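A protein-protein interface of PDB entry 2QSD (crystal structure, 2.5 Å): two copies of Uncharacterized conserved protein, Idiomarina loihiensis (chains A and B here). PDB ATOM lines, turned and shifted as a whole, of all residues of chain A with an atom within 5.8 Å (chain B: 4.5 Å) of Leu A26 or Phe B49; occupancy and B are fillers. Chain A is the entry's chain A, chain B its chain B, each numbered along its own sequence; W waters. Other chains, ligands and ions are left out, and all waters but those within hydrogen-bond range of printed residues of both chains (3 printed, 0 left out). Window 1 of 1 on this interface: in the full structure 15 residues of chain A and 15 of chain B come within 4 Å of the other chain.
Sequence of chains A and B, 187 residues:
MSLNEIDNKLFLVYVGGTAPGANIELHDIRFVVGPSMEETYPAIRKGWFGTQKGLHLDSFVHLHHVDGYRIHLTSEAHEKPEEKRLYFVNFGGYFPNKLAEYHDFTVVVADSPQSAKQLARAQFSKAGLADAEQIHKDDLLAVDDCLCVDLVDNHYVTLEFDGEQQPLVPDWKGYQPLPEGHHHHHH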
ATOM      1  N   VAL A  15     -33.527  18.081  -5.707  1.00  0.00           N
ATOM      2  CA  VAL A  15     -32.986  18.540  -4.436  1.00  0.00           C
ATOM      3  C   VAL A  15     -31.764  17.731  -4.049  1.00  0.00           C
ATOM      4  O   VAL A  15     -31.573  16.613  -4.528  1.00  0.00           O
ATOM      5  CB  VAL A  15     -34.042  18.513  -3.316  1.00  0.00           C
ATOM      6  CG1 VAL A  15     -35.124  19.525  -3.603  1.00  0.00           C
ATOM      7  CG2 VAL A  15     -34.657  17.123  -3.170  1.00  0.00           C
ATOM      8  N   GLY A  16     -30.935  18.309  -3.188  1.00  0.00           N
ATOM      9  CA  GLY A  16     -29.681  17.692  -2.782  1.00  0.00           C
ATOM     10  C   GLY A  16     -29.402  17.853  -1.305  1.00  0.00           C
ATOM     11  O   GLY A  16     -29.910  18.771  -0.649  1.00  0.00           O
ATOM     12  N   GLY A  17     -28.579  16.956  -0.782  1.00  0.00           N
ATOM     13  CA  GLY A  17     -28.231  16.980   0.624  1.00  0.00           C
ATOM     14  C   GLY A  17     -27.551  15.700   1.050  1.00  0.00           C
ATOM     15  O   GLY A  17     -27.096  14.911   0.216  1.00  0.00           O
ATOM     16  N   THR A  18     -27.497  15.488   2.357  1.00  0.00           N
ATOM     17  CA  THR A  18     -26.788  14.348   2.902  1.00  0.00           C
ATOM     18  C   THR A  18     -27.741  13.322   3.535  1.00  0.00           C
ATOM     19  O   THR A  18     -28.916  13.614   3.778  1.00  0.00           O
ATOM     20  CB  THR A  18     -25.663  14.815   3.878  1.00  0.00           C
ATOM     21  OG1 THR A  18     -24.862  13.694   4.256  1.00  0.00           O
ATOM     22  CG2 THR A  18     -26.238  15.464   5.126  1.00  0.00           C
ATOM     23  N   ALA A  19     -27.235  12.113   3.751  1.00  0.00           N
ATOM     24  CA  ALA A  19     -27.932  11.085   4.528  1.00  0.00           C
ATOM     25  C   ALA A  19     -26.904  10.307   5.358  1.00  0.00           C
ATOM     26  O   ALA A  19     -25.737  10.225   4.956  1.00  0.00           O
ATOM     27  CB  ALA A  19     -28.706  10.147   3.609  1.00  0.00           C
ATOM     28  N   PRO A  20     -27.317   9.753   6.521  1.00  0.00           N
ATOM     29  CA  PRO A  20     -26.363   9.020   7.364  1.00  0.00           C
ATOM     30  C   PRO A  20     -25.764   7.803   6.673  1.00  0.00           C
ATOM     31  O   PRO A  20     -26.486   7.019   6.046  1.00  0.00           O
ATOM     32  CB  PRO A  20     -27.219   8.575   8.549  1.00  0.00           C
ATOM     33  CG  PRO A  20     -28.357   9.555   8.586  1.00  0.00           C
ATOM     34  CD  PRO A  20     -28.656   9.792   7.142  1.00  0.00           C
ATOM     35  N   GLY A  21     -24.445   7.671   6.774  1.00  0.00           N
ATOM     36  CA  GLY A  21     -23.734   6.561   6.151  1.00  0.00           C
ATOM     37  C   GLY A  21     -23.160   6.851   4.780  1.00  0.00           C
ATOM     38  O   GLY A  21     -22.175   6.236   4.383  1.00  0.00           O
ATOM     39  N   ALA A  22     -23.775   7.777   4.050  1.00  0.00           N
ATOM     40  CA  ALA A  22     -23.276   8.161   2.733  1.00  0.00           C
ATOM     41  C   ALA A  22     -22.074   9.099   2.830  1.00  0.00           C
ATOM     42  O   ALA A  22     -22.040   9.996   3.676  1.00  0.00           O
ATOM     43  CB  ALA A  22     -24.381   8.790   1.911  1.00  0.00           C
ATOM     44  N   ILE A  24     -20.914  10.941   0.021  1.00  0.00           N
ATOM     45  CA  ILE A  24     -21.138  12.109  -0.825  1.00  0.00           C
ATOM     46  C   ILE A  24     -22.570  12.616  -0.724  1.00  0.00           C
ATOM     47  O   ILE A  24     -23.435  11.948  -0.165  1.00  0.00           O
ATOM     48  CB  ILE A  24     -20.748  11.855  -2.311  1.00  0.00           C
ATOM     49  CG1 ILE A  24     -21.687  10.843  -2.977  1.00  0.00           C
ATOM     50  CG2 ILE A  24     -19.289  11.419  -2.421  1.00  0.00           C
ATOM     51  CD1 ILE A  24     -21.407  10.641  -4.456  1.00  0.00           C
ATOM     52  N   GLU A  25     -22.788  13.816  -1.246  1.00  0.00           N
ATOM     53  CA  GLU A  25     -24.106  14.426  -1.364  1.00  0.00           C
ATOM     54  C   GLU A  25     -24.976  13.575  -2.294  1.00  0.00           C
ATOM     55  O   GLU A  25     -24.517  13.106  -3.338  1.00  0.00           O
ATOM     56  CB  GLU A  25     -23.948  15.836  -1.950  1.00  0.00           C
ATOM     57  CG  GLU A  25     -25.006  16.849  -1.552  1.00  0.00           C
ATOM     58  CD  GLU A  25     -24.583  17.735  -0.389  1.00  0.00           C
ATOM     59  OE1 GLU A  25     -25.162  18.828  -0.237  1.00  0.00           O
ATOM     60  OE2 GLU A  25     -23.677  17.352   0.372  1.00  0.00           O
ATOM     61  N   LEU A  26     -26.225  13.360  -1.905  1.00  0.00           N
ATOM     62  CA  LEU A  26     -27.149  12.585  -2.723  1.00  0.00           C
ATOM     63  C   LEU A  26     -28.215  13.509  -3.274  1.00  0.00           C
ATOM     64  O   LEU A  26     -28.409  14.613  -2.756  1.00  0.00           O
ATOM     65  CB  LEU A  26     -27.796  11.473  -1.898  1.00  0.00           C
ATOM     66  CG  LEU A  26     -26.827  10.774  -0.952  1.00  0.00           C
ATOM     67  CD1 LEU A  26     -27.575  10.212   0.222  1.00  0.00           C
ATOM     68  CD2 LEU A  26     -26.014   9.703  -1.667  1.00  0.00           C
ATOM     69  N   HIS A  27     -28.898  13.057  -4.323  1.00  0.00           N
ATOM     70  CA  HIS A  27     -29.934  13.850  -4.975  1.00  0.00           C
ATOM     71  C   HIS A  27     -31.196  13.031  -5.233  1.00  0.00           C
ATOM     72  O   HIS A  27     -31.114  11.857  -5.565  1.00  0.00           O
ATOM     73  CB  HIS A  27     -29.412  14.415  -6.297  1.00  0.00           C
ATOM     74  CG  HIS A  27     -28.252  15.345  -6.137  1.00  0.00           C
ATOM     75  ND1 HIS A  27     -26.953  14.900  -6.018  1.00  0.00           N
ATOM     76  CD2 HIS A  27     -28.198  16.696  -6.062  1.00  0.00           C
ATOM     77  CE1 HIS A  27     -26.148  15.936  -5.878  1.00  0.00           C
ATOM     78  NE2 HIS A  27     -26.878  17.037  -5.900  1.00  0.00           N
ATOM     79  N   ASP A  28     -32.354  13.667  -5.098  1.00  0.00           N
ATOM     80  CA  ASP A  28     -33.633  13.039  -5.422  1.00  0.00           C
ATOM     81  C   ASP A  28     -34.533  14.017  -6.187  1.00  0.00           C
ATOM     82  O   ASP A  28     -34.348  15.232  -6.107  1.00  0.00           O
ATOM     83  CB  ASP A  28     -34.335  12.552  -4.140  1.00  0.00           C
ATOM     84  CG  ASP A  28     -35.482  11.583  -4.417  1.00  0.00           C
ATOM     85  OD1 ASP A  28     -35.475  10.943  -5.487  1.00  0.00           O
ATOM     86  OD2 ASP A  28     -36.389  11.453  -3.564  1.00  0.00           O
ATOM     87  N   TRP A  48     -38.023  14.820   1.479  1.00  0.00           N
ATOM     88  CA  TRP A  48     -36.589  14.490   1.469  1.00  0.00           C
ATOM     89  C   TRP A  48     -36.289  13.321   2.399  1.00  0.00           C
ATOM     90  O   TRP A  48     -36.618  13.365   3.572  1.00  0.00           O
ATOM     91  CB  TRP A  48     -35.744  15.715   1.850  1.00  0.00           C
ATOM     92  CG  TRP A  48     -34.278  15.435   1.994  1.00  0.00           C
ATOM     93  CD1 TRP A  48     -33.537  15.539   3.136  1.00  0.00           C
ATOM     94  CD2 TRP A  48     -33.366  15.017   0.963  1.00  0.00           C
ATOM     95  NE1 TRP A  48     -32.228  15.218   2.882  1.00  0.00           N
ATOM     96  CE2 TRP A  48     -32.095  14.884   1.561  1.00  0.00           C
ATOM     97  CE3 TRP A  48     -33.499  14.745  -0.404  1.00  0.00           C
ATOM     98  CZ2 TRP A  48     -30.966  14.485   0.845  1.00  0.00           C
ATOM     99  CZ3 TRP A  48     -32.371  14.344  -1.117  1.00  0.00           C
ATOM    100  CH2 TRP A  48     -31.126  14.219  -0.490  1.00  0.00           C
ATOM    101  N   PHE A  49     -35.675  12.278   1.855  1.00  0.00           N
ATOM    102  CA  PHE A  49     -35.489  11.013   2.566  1.00  0.00           C
ATOM    103  C   PHE A  49     -34.354  11.071   3.586  1.00  0.00           C
ATOM    104  O   PHE A  49     -34.302  10.254   4.511  1.00  0.00           O
ATOM    105  CB  PHE A  49     -35.214   9.884   1.558  1.00  0.00           C
ATOM    106  CG  PHE A  49     -33.836   9.930   0.966  1.00  0.00           C
ATOM    107  CD1 PHE A  49     -33.559  10.771  -0.109  1.00  0.00           C
ATOM    108  CD2 PHE A  49     -32.801   9.147   1.498  1.00  0.00           C
ATOM    109  CE1 PHE A  49     -32.284  10.823  -0.655  1.00  0.00           C
ATOM    110  CE2 PHE A  49     -31.522   9.205   0.966  1.00  0.00           C
ATOM    111  CZ  PHE A  49     -31.260  10.042  -0.113  1.00  0.00           C
ATOM    112  N   ALA B  19     -33.125   3.726  -2.213  1.00  0.00           N
ATOM    113  CA  ALA B  19     -33.263   3.866  -0.773  1.00  0.00           C
ATOM    114  C   ALA B  19     -34.711   4.196  -0.474  1.00  0.00           C
ATOM    115  O   ALA B  19     -35.376   4.830  -1.296  1.00  0.00           O
ATOM    116  CB  ALA B  19     -32.350   4.954  -0.242  1.00  0.00           C
ATOM    117  N   LEU B  26     -29.967   6.427  -6.268  1.00  0.00           N
ATOM    118  CA  LEU B  26     -28.949   7.231  -5.612  1.00  0.00           C
ATOM    119  C   LEU B  26     -27.586   6.625  -5.890  1.00  0.00           C
ATOM    120  O   LEU B  26     -27.495   5.470  -6.307  1.00  0.00           O
ATOM    121  CB  LEU B  26     -29.226   7.311  -4.115  1.00  0.00           C
ATOM    122  CG  LEU B  26     -30.702   7.633  -3.854  1.00  0.00           C
ATOM    123  CD1 LEU B  26     -31.080   7.233  -2.483  1.00  0.00           C
ATOM    124  CD2 LEU B  26     -30.996   9.102  -4.077  1.00  0.00           C
ATOM    125  N   HIS B  27     -26.535   7.416  -5.684  1.00  0.00           N
ATOM    126  CA  HIS B  27     -25.174   6.957  -5.918  1.00  0.00           C
ATOM    127  C   HIS B  27     -24.256   7.378  -4.787  1.00  0.00           C
ATOM    128  O   HIS B  27     -24.376   8.479  -4.271  1.00  0.00           O
ATOM    129  CB  HIS B  27     -24.641   7.531  -7.229  1.00  0.00           C
ATOM    130  CG  HIS B  27     -25.485   7.199  -8.414  1.00  0.00           C
ATOM    131  ND1 HIS B  27     -25.346   6.023  -9.118  1.00  0.00           N
ATOM    132  CD2 HIS B  27     -26.500   7.877  -9.002  1.00  0.00           C
ATOM    133  CE1 HIS B  27     -26.236   5.991 -10.093  1.00  0.00           C
ATOM    134  NE2 HIS B  27     -26.947   7.104 -10.045  1.00  0.00           N
ATOM    135  N   GLY B  47     -21.234  -0.951   3.525  1.00  0.00           N
ATOM    136  CA  GLY B  47     -21.001   0.482   3.381  1.00  0.00           C
ATOM    137  C   GLY B  47     -22.207   1.199   2.790  1.00  0.00           C
ATOM    138  O   GLY B  47     -22.461   2.359   3.115  1.00  0.00           O
ATOM    139  N   TRP B  48     -22.952   0.501   1.931  1.00  0.00           N
ATOM    140  CA  TRP B  48     -24.131   1.064   1.262  1.00  0.00           C
ATOM    141  C   TRP B  48     -25.287   1.325   2.231  1.00  0.00           C
ATOM    142  O   TRP B  48     -25.759   0.416   2.915  1.00  0.00           O
ATOM    143  CB  TRP B  48     -24.580   0.152   0.109  1.00  0.00           C
ATOM    144  CG  TRP B  48     -25.863   0.570  -0.553  1.00  0.00           C
ATOM    145  CD1 TRP B  48     -27.053  -0.083  -0.496  1.00  0.00           C
ATOM    146  CD2 TRP B  48     -26.085   1.740  -1.360  1.00  0.00           C
ATOM    147  NE1 TRP B  48     -28.001   0.594  -1.219  1.00  0.00           N
ATOM    148  CE2 TRP B  48     -27.439   1.720  -1.756  1.00  0.00           C
ATOM    149  CE3 TRP B  48     -25.269   2.799  -1.792  1.00  0.00           C
ATOM    150  CZ2 TRP B  48     -28.006   2.718  -2.563  1.00  0.00           C
ATOM    151  CZ3 TRP B  48     -25.830   3.793  -2.597  1.00  0.00           C
ATOM    152  CH2 TRP B  48     -27.185   3.742  -2.973  1.00  0.00           C
ATOM    153  N   PHE B  49     -25.742   2.573   2.269  1.00  0.00           N
ATOM    154  CA  PHE B  49     -26.754   3.006   3.229  1.00  0.00           C
ATOM    155  C   PHE B  49     -28.182   2.578   2.883  1.00  0.00           C
ATOM    156  O   PHE B  49     -29.040   2.529   3.763  1.00  0.00           O
ATOM    157  CB  PHE B  49     -26.709   4.531   3.391  1.00  0.00           C
ATOM    158  CG  PHE B  49     -27.313   5.285   2.237  1.00  0.00           C
ATOM    159  CD1 PHE B  49     -26.570   5.532   1.081  1.00  0.00           C
ATOM    160  CD2 PHE B  49     -28.624   5.753   2.303  1.00  0.00           C
ATOM    161  CE1 PHE B  49     -27.128   6.221   0.012  1.00  0.00           C
ATOM    162  CE2 PHE B  49     -29.187   6.441   1.232  1.00  0.00           C
ATOM    163  CZ  PHE B  49     -28.440   6.673   0.091  1.00  0.00           C
ATOM    164  N   GLY B  50     -28.442   2.305   1.608  1.00  0.00           N
ATOM    165  CA  GLY B  50     -29.814   2.125   1.141  1.00  0.00           C
ATOM    166  C   GLY B  50     -30.261   0.681   1.075  1.00  0.00           C
ATOM    167  O   GLY B  50     -29.762  -0.174   1.811  1.00  0.00           O
HETATM  168  O   HOH W   1     -24.912  10.954  -5.215  1.00  0.00           O
HETATM  169  O   HOH W   2     -27.689  10.464  -5.390  1.00  0.00           O
HETATM  170  O   HOH W   3     -22.728   3.411   5.496  1.00  0.00           O
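The backbone carbonyl oxygen (O) of Gly A17 lies within hydrogen-bond range of the backbone NH (N) of Leu A26.
Leu A26 touches His B27, and with the chains exchanged His A27 touches Leu B26.
Leu A26 touches Phe B49, and with the chains exchanged Phe A49 touches Leu B26.
Phe A49 touches its own counterpart, Phe B49.
Of the 7 pairs that touch across the chains among the printed residues, 5 have their exchanged pair printed and touching as well.
Water W3 lies within hydrogen-bond range of the backbone carbonyl oxygen of Gly B47 (2.6 Å) and the backbone carbonyl oxygen of Gly A21 (3.1 Å).
Water W1 lies within hydrogen-bond range of O of His B27 (2.7 Å) and O of Glu A25 (2.9 Å).
Water W2 bridges N of His A27 (3.1 Å) and N of His B27 (3.3 Å).
Phe B49 touches Pro A20 (CB to O, 3.6 Å).
Ile A24 touches His B27.
Leu A26 touches His B27.
CZ of Phe B49 touches CD1 of Leu A26, at 3.6 Å.
His A27 touches Leu B26 (O to CD2, 3.1 Å).
CZ of Phe A49 touches CD1 of Leu B26, at 3.7 Å.
CE2 of Phe A49 touches CE2 of Phe B49, 3.6 Å away.
Hydrophobic or aromatic side chains of chain B within 4 Å of the printed part of chain A: Leu B26 and Phe B49.
Printed residues of chain A that touch a printed residue of chain B: Pro A20, Ile A24, Leu A26, His A27 and Phe A49.
Hydrophobic or aromatic side chains of chain A that line the printed part of chain B: Ile A24, Leu A26 and Phe A49.
Among the printed residues, no Asp or Glu carboxylate lies within 4 Å of a Lys or Arg side-chain nitrogen of the other chain.
Of chain B, only His B27 (3.3 Å) and Phe B49 (3.6 Å) come within 4 Å of Leu A26.
Of the printed residues of chain A, Phe B49 touches Pro A20, Leu A26 and Phe A49.
Of the printed residues of chain B, His A27 touches Leu B26.
Of the printed residues of chain A, His B27 touches Ile A24 and Leu A26.
Glu A25 touches none of the printed residues of chain B.
Gly A16 touches none of the printed residues of chain B.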
